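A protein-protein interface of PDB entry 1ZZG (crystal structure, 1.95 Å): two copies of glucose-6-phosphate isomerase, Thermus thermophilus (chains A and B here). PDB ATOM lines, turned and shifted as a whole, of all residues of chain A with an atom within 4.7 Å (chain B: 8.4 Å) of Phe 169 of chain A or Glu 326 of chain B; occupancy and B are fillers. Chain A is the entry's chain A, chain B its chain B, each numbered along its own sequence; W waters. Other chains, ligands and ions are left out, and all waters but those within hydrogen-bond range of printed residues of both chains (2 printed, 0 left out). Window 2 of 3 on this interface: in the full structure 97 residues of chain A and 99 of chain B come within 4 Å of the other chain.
Val 325 of chain B touches Leu 140 of chain A (CG1 to CD1, 3.4 Å). CD1 of Leu 328 of chain B touches O of Pro 165 of chain A, at 3.8 Å. Glu 326 of chain B touches Phe 169 of chain A (O to CE1, 3.7 Å). Phe 169 of chain A touches Gly 327 of chain B. CD1 of Leu 328 of chain B touches CB of Phe 169 of chain A, at 3.9 Å. Arg 172 of chain A touches Gly 327 of chain B (NE to CA, 3.3 Å).
Water W1 lies within hydrogen-bond range of O of Pro 165 of chain A (2.6 Å) and O of Gly 327 of chain B (3.4 Å). Water W2 bridges OE2 of Glu 173 of chain A (2.9 Å) and O of Glu 326 of chain B (3.1 Å).
No position is printed for both chains.
NH2 of Arg 172 of chain A lies within salt-bridge range of OE2 of Glu 326 of chain B.
Arg 167 of chain A touches none of the printed residues of chain B. No residue of chain B comes within 4 Å of Ala 168 of chain A. No residue of chain B comes within 4 Å of Ala 170 of chain A. Printed residues of chain B within 4 Å of Arg 172 of chain A: Glu 326 (3.7 Å) and Gly 327 (3.3 Å). Leu 175 of chain A touches none of the printed residues of chain B. Glu 326 of chain B touches just these residues of chain A: Phe 169 (3.7 Å) and Arg 172 (3.7 Å). Printed residues of chain A within 4 Å of Gly 327 of chain B: Phe 169 and Arg 172. The nearest printed residue of chain B that does not touch Pro 165 of chain A is Gly 327 of chain B (5.4 Å).
The guanidinium group of Arg 172 of chain A is in salt-bridge range of the side-chain carboxylate of Glu 173 of chain A, 3.7 Å away.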
ATOM      1  N   LEU A 140     -24.411  13.026 -13.503  1.00  0.00           N
ATOM      2  CA  LEU A 140     -25.167  14.196 -13.931  1.00  0.00           C
ATOM      3  C   LEU A 140     -26.569  14.167 -13.319  1.00  0.00           C
ATOM      4  O   LEU A 140     -27.029  15.164 -12.767  1.00  0.00           O
ATOM      5  CB  LEU A 140     -25.246  14.236 -15.449  1.00  0.00           C
ATOM      6  CG  LEU A 140     -24.287  15.214 -16.132  1.00  0.00           C
ATOM      7  CD1 LEU A 140     -24.438  15.109 -17.633  1.00  0.00           C
ATOM      8  CD2 LEU A 140     -24.583  16.629 -15.664  1.00  0.00           C
ATOM      9  N   TRP A 151     -26.091  22.905 -10.004  1.00  0.00           N
ATOM     10  CA  TRP A 151     -25.334  21.729 -10.422  1.00  0.00           C
ATOM     11  C   TRP A 151     -24.135  22.064 -11.306  1.00  0.00           C
ATOM     12  O   TRP A 151     -23.062  21.484 -11.148  1.00  0.00           O
ATOM     13  CB  TRP A 151     -26.234  20.713 -11.146  1.00  0.00           C
ATOM     14  CG  TRP A 151     -26.700  21.111 -12.526  1.00  0.00           C
ATOM     15  CD1 TRP A 151     -27.845  21.788 -12.842  1.00  0.00           C
ATOM     16  CD2 TRP A 151     -26.047  20.822 -13.773  1.00  0.00           C
ATOM     17  NE1 TRP A 151     -27.949  21.933 -14.204  1.00  0.00           N
ATOM     18  CE2 TRP A 151     -26.862  21.351 -14.803  1.00  0.00           C
ATOM     19  CE3 TRP A 151     -24.855  20.166 -14.122  1.00  0.00           C
ATOM     20  CZ2 TRP A 151     -26.522  21.247 -16.165  1.00  0.00           C
ATOM     21  CZ3 TRP A 151     -24.515  20.062 -15.476  1.00  0.00           C
ATOM     22  CH2 TRP A 151     -25.349  20.601 -16.479  1.00  0.00           C
ATOM     23  N   LEU A 155     -19.611  20.607 -11.716  1.00  0.00           N
ATOM     24  CA  LEU A 155     -19.091  19.792 -12.812  1.00  0.00           C
ATOM     25  C   LEU A 155     -18.091  20.586 -13.646  1.00  0.00           C
ATOM     26  O   LEU A 155     -18.423  21.631 -14.212  1.00  0.00           O
ATOM     27  CB  LEU A 155     -20.228  19.300 -13.714  1.00  0.00           C
ATOM     28  CG  LEU A 155     -19.786  18.497 -14.946  1.00  0.00           C
ATOM     29  CD1 LEU A 155     -19.062  17.233 -14.505  1.00  0.00           C
ATOM     30  CD2 LEU A 155     -20.999  18.143 -15.796  1.00  0.00           C
ATOM     31  N   PRO A 165     -17.467  15.216 -27.857  1.00  0.00           N
ATOM     32  CA  PRO A 165     -18.745  15.517 -27.209  1.00  0.00           C
ATOM     33  C   PRO A 165     -18.645  16.224 -25.856  1.00  0.00           C
ATOM     34  O   PRO A 165     -19.543  16.988 -25.488  1.00  0.00           O
ATOM     35  CB  PRO A 165     -19.423  14.145 -27.127  1.00  0.00           C
ATOM     36  CG  PRO A 165     -18.281  13.186 -27.087  1.00  0.00           C
ATOM     37  CD  PRO A 165     -17.323  13.769 -28.092  1.00  0.00           C
ATOM     38  N   LEU A 166     -17.565  15.984 -25.116  1.00  0.00           N
ATOM     39  CA  LEU A 166     -17.394  16.633 -23.816  1.00  0.00           C
ATOM     40  C   LEU A 166     -17.165  18.127 -23.986  1.00  0.00           C
ATOM     41  O   LEU A 166     -17.658  18.935 -23.201  1.00  0.00           O
ATOM     42  CB  LEU A 166     -16.212  16.037 -23.049  1.00  0.00           C
ATOM     43  CG  LEU A 166     -16.460  14.786 -22.214  1.00  0.00           C
ATOM     44  CD1 LEU A 166     -15.233  14.515 -21.364  1.00  0.00           C
ATOM     45  CD2 LEU A 166     -17.678  14.985 -21.322  1.00  0.00           C
ATOM     46  N   ARG A 167     -16.396  18.490 -25.003  1.00  0.00           N
ATOM     47  CA  ARG A 167     -16.126  19.895 -25.271  1.00  0.00           C
ATOM     48  C   ARG A 167     -17.440  20.587 -25.641  1.00  0.00           C
ATOM     49  O   ARG A 167     -17.746  21.668 -25.145  1.00  0.00           O
ATOM     50  CB  ARG A 167     -15.121  20.029 -26.418  1.00  0.00           C
ATOM     51  CG  ARG A 167     -14.876  21.466 -26.891  1.00  0.00           C
ATOM     52  CD  ARG A 167     -14.469  22.389 -25.753  1.00  0.00           C
ATOM     53  NE  ARG A 167     -13.295  21.905 -25.029  1.00  0.00           N
ATOM     54  CZ  ARG A 167     -12.673  22.596 -24.076  1.00  0.00           C
ATOM     55  NH1 ARG A 167     -13.113  23.800 -23.734  1.00  0.00           N
ATOM     56  NH2 ARG A 167     -11.611  22.089 -23.465  1.00  0.00           N
ATOM     57  N   ALA A 168     -18.214  19.947 -26.510  1.00  0.00           N
ATOM     58  CA  ALA A 168     -19.489  20.501 -26.950  1.00  0.00           C
ATOM     59  C   ALA A 168     -20.460  20.636 -25.781  1.00  0.00           C
ATOM     60  O   ALA A 168     -21.154  21.650 -25.656  1.00  0.00           O
ATOM     61  CB  ALA A 168     -20.089  19.620 -28.035  1.00  0.00           C
ATOM     62  N   PHE A 169     -20.496  19.615 -24.927  1.00  0.00           N
ATOM     63  CA  PHE A 169     -21.372  19.601 -23.756  1.00  0.00           C
ATOM     64  C   PHE A 169     -21.025  20.714 -22.772  1.00  0.00           C
ATOM     65  O   PHE A 169     -21.910  21.351 -22.196  1.00  0.00           O
ATOM     66  CB  PHE A 169     -21.270  18.255 -23.035  1.00  0.00           C
ATOM     67  CG  PHE A 169     -22.208  18.127 -21.869  1.00  0.00           C
ATOM     68  CD1 PHE A 169     -23.585  18.078 -22.073  1.00  0.00           C
ATOM     69  CD2 PHE A 169     -21.721  18.066 -20.567  1.00  0.00           C
ATOM     70  CE1 PHE A 169     -24.465  17.971 -20.997  1.00  0.00           C
ATOM     71  CE2 PHE A 169     -22.591  17.960 -19.480  1.00  0.00           C
ATOM     72  CZ  PHE A 169     -23.966  17.913 -19.698  1.00  0.00           C
ATOM     73  N   ALA A 170     -19.732  20.936 -22.571  1.00  0.00           N
ATOM     74  CA  ALA A 170     -19.274  21.969 -21.656  1.00  0.00           C
ATOM     75  C   ALA A 170     -19.670  23.355 -22.166  1.00  0.00           C
ATOM     76  O   ALA A 170     -20.088  24.213 -21.387  1.00  0.00           O
ATOM     77  CB  ALA A 170     -17.756  21.881 -21.481  1.00  0.00           C
ATOM     78  N   GLU A 171     -19.548  23.567 -23.473  1.00  0.00           N
ATOM     79  CA  GLU A 171     -19.895  24.859 -24.060  1.00  0.00           C
ATOM     80  C   GLU A 171     -21.407  25.086 -24.059  1.00  0.00           C
ATOM     81  O   GLU A 171     -21.872  26.204 -23.837  1.00  0.00           O
ATOM     82  CB  GLU A 171     -19.335  24.960 -25.484  1.00  0.00           C
ATOM     83  CG  GLU A 171     -17.822  24.822 -25.533  1.00  0.00           C
ATOM     84  CD  GLU A 171     -17.243  25.006 -26.926  1.00  0.00           C
ATOM     85  OE1 GLU A 171     -17.769  24.405 -27.885  1.00  0.00           O
ATOM     86  OE2 GLU A 171     -16.245  25.747 -27.054  1.00  0.00           O
ATOM     87  N   ARG A 172     -22.165  24.020 -24.300  1.00  0.00           N
ATOM     88  CA  ARG A 172     -23.623  24.095 -24.305  1.00  0.00           C
ATOM     89  C   ARG A 172     -24.166  24.444 -22.919  1.00  0.00           C
ATOM     90  O   ARG A 172     -25.062  25.273 -22.782  1.00  0.00           O
ATOM     91  CB  ARG A 172     -24.215  22.754 -24.746  1.00  0.00           C
ATOM     92  CG  ARG A 172     -25.715  22.629 -24.520  1.00  0.00           C
ATOM     93  CD  ARG A 172     -26.159  21.171 -24.541  1.00  0.00           C
ATOM     94  NE  ARG A 172     -27.590  21.007 -24.282  1.00  0.00           N
ATOM     95  CZ  ARG A 172     -28.557  21.439 -25.089  1.00  0.00           C
ATOM     96  NH1 ARG A 172     -28.256  22.071 -26.216  1.00  0.00           N
ATOM     97  NH2 ARG A 172     -29.829  21.225 -24.775  1.00  0.00           N
ATOM     98  N   GLU A 173     -23.612  23.807 -21.894  1.00  0.00           N
ATOM     99  CA  GLU A 173     -24.052  24.015 -20.520  1.00  0.00           C
ATOM    100  C   GLU A 173     -23.344  25.129 -19.754  1.00  0.00           C
ATOM    101  O   GLU A 173     -23.723  25.441 -18.623  1.00  0.00           O
ATOM    102  CB  GLU A 173     -23.916  22.710 -19.737  1.00  0.00           C
ATOM    103  CG  GLU A 173     -24.818  21.588 -20.225  1.00  0.00           C
ATOM    104  CD  GLU A 173     -26.298  21.909 -20.066  1.00  0.00           C
ATOM    105  OE1 GLU A 173     -26.635  22.870 -19.342  1.00  0.00           O
ATOM    106  OE2 GLU A 173     -27.127  21.189 -20.663  1.00  0.00           O
ATOM    107  N   LEU A 175     -20.144  25.143 -18.699  1.00  0.00           N
ATOM    108  CA  LEU A 175     -19.346  24.521 -17.652  1.00  0.00           C
ATOM    109  C   LEU A 175     -17.897  24.965 -17.735  1.00  0.00           C
ATOM    110  O   LEU A 175     -17.395  25.273 -18.818  1.00  0.00           O
ATOM    111  CB  LEU A 175     -19.396  22.997 -17.790  1.00  0.00           C
ATOM    112  CG  LEU A 175     -20.789  22.375 -17.882  1.00  0.00           C
ATOM    113  CD1 LEU A 175     -20.663  20.877 -18.084  1.00  0.00           C
ATOM    114  CD2 LEU A 175     -21.582  22.695 -16.620  1.00  0.00           C
ATOM    115  N   PRO B 323     -28.662   6.705 -17.196  1.00  0.00           N
ATOM    116  CA  PRO B 323     -29.705   7.669 -17.557  1.00  0.00           C
ATOM    117  C   PRO B 323     -29.363   8.523 -18.774  1.00  0.00           C
ATOM    118  O   PRO B 323     -28.192   8.699 -19.121  1.00  0.00           O
ATOM    119  CB  PRO B 323     -29.851   8.497 -16.287  1.00  0.00           C
ATOM    120  CG  PRO B 323     -28.439   8.584 -15.810  1.00  0.00           C
ATOM    121  CD  PRO B 323     -27.909   7.168 -16.017  1.00  0.00           C
ATOM    122  N   GLU B 324     -30.392   9.043 -19.432  1.00  0.00           N
ATOM    123  CA  GLU B 324     -30.174   9.870 -20.599  1.00  0.00           C
ATOM    124  C   GLU B 324     -29.651  11.240 -20.197  1.00  0.00           C
ATOM    125  O   GLU B 324     -29.922  11.758 -19.122  1.00  0.00           O
ATOM    126  CB  GLU B 324     -31.492  10.012 -21.373  1.00  0.00           C
ATOM    127  CG  GLU B 324     -32.685  10.379 -20.483  1.00  0.00           C
ATOM    128  CD  GLU B 324     -33.886  10.677 -21.358  1.00  0.00           C
ATOM    129  OE1 GLU B 324     -34.243   9.837 -22.174  1.00  0.00           O
ATOM    130  OE2 GLU B 324     -34.449  11.760 -21.223  1.00  0.00           O
ATOM    131  N   VAL B 325     -28.830  11.797 -21.093  1.00  0.00           N
ATOM    132  CA  VAL B 325     -28.300  13.122 -20.856  1.00  0.00           C
ATOM    133  C   VAL B 325     -28.680  14.075 -21.982  1.00  0.00           C
ATOM    134  O   VAL B 325     -28.349  13.878 -23.145  1.00  0.00           O
ATOM    135  CB  VAL B 325     -26.785  13.005 -20.752  1.00  0.00           C
ATOM    136  CG1 VAL B 325     -26.182  14.371 -20.442  1.00  0.00           C
ATOM    137  CG2 VAL B 325     -26.431  12.027 -19.644  1.00  0.00           C
ATOM    138  N   GLU B 326     -29.456  15.106 -21.616  1.00  0.00           N
ATOM    139  CA  GLU B 326     -29.830  16.109 -22.599  1.00  0.00           C
ATOM    140  C   GLU B 326     -28.610  16.929 -23.027  1.00  0.00           C
ATOM    141  O   GLU B 326     -27.875  17.470 -22.214  1.00  0.00           O
ATOM    142  CB  GLU B 326     -30.867  17.021 -21.953  1.00  0.00           C
ATOM    143  CG  GLU B 326     -31.565  17.932 -22.961  1.00  0.00           C
ATOM    144  CD  GLU B 326     -31.783  19.283 -22.327  1.00  0.00           C
ATOM    145  OE1 GLU B 326     -31.068  19.605 -21.389  1.00  0.00           O
ATOM    146  OE2 GLU B 326     -32.680  19.999 -22.766  1.00  0.00           O
ATOM    147  N   GLY B 327     -28.378  16.968 -24.352  1.00  0.00           N
ATOM    148  CA  GLY B 327     -27.254  17.754 -24.855  1.00  0.00           C
ATOM    149  C   GLY B 327     -25.996  16.903 -25.057  1.00  0.00           C
ATOM    150  O   GLY B 327     -24.936  17.388 -25.424  1.00  0.00           O
ATOM    151  N   LEU B 328     -26.125  15.595 -24.759  1.00  0.00           N
ATOM    152  CA  LEU B 328     -24.991  14.696 -24.972  1.00  0.00           C
ATOM    153  C   LEU B 328     -25.401  13.476 -25.797  1.00  0.00           C
ATOM    154  O   LEU B 328     -25.331  12.339 -25.350  1.00  0.00           O
ATOM    155  CB  LEU B 328     -24.470  14.247 -23.606  1.00  0.00           C
ATOM    156  CG  LEU B 328     -23.123  13.520 -23.688  1.00  0.00           C
ATOM    157  CD1 LEU B 328     -21.962  14.483 -23.957  1.00  0.00           C
ATOM    158  CD2 LEU B 328     -22.774  12.784 -22.391  1.00  0.00           C
ATOM    159  N   GLU B 329     -25.876  13.741 -27.009  1.00  0.00           N
ATOM    160  CA  GLU B 329     -26.374  12.703 -27.901  1.00  0.00           C
ATOM    161  C   GLU B 329     -25.323  11.676 -28.301  1.00  0.00           C
ATOM    162  O   GLU B 329     -25.657  10.552 -28.674  1.00  0.00           O
ATOM    163  CB  GLU B 329     -26.957  13.334 -29.172  1.00  0.00           C
ATOM    164  CG  GLU B 329     -28.053  14.369 -28.938  1.00  0.00           C
ATOM    165  CD  GLU B 329     -27.520  15.719 -28.466  1.00  0.00           C
ATOM    166  OE1 GLU B 329     -26.283  15.919 -28.452  1.00  0.00           O
ATOM    167  OE2 GLU B 329     -28.346  16.592 -28.117  1.00  0.00           O
ATOM    168  N   PHE B 335     -27.561   5.101 -23.168  1.00  0.00           N
ATOM    169  CA  PHE B 335     -28.804   5.356 -22.443  1.00  0.00           C
ATOM    170  C   PHE B 335     -29.702   4.128 -22.449  1.00  0.00           C
ATOM    171  O   PHE B 335     -29.884   3.491 -23.486  1.00  0.00           O
ATOM    172  CB  PHE B 335     -29.569   6.534 -23.056  1.00  0.00           C
ATOM    173  CG  PHE B 335     -28.778   7.814 -23.136  1.00  0.00           C
ATOM    174  CD1 PHE B 335     -27.672   8.027 -22.315  1.00  0.00           C
ATOM    175  CD2 PHE B 335     -29.158   8.821 -24.023  1.00  0.00           C
ATOM    176  CE1 PHE B 335     -26.958   9.221 -22.377  1.00  0.00           C
ATOM    177  CE2 PHE B 335     -28.452  10.020 -24.093  1.00  0.00           C
ATOM    178  CZ  PHE B 335     -27.349  10.221 -23.269  1.00  0.00           C
HETATM  179  O   HOH W   1     -21.857  16.708 -26.688  1.00  0.00           O
HETATM  180  O   HOH W   2     -27.579  18.584 -19.355  1.00  0.00           O
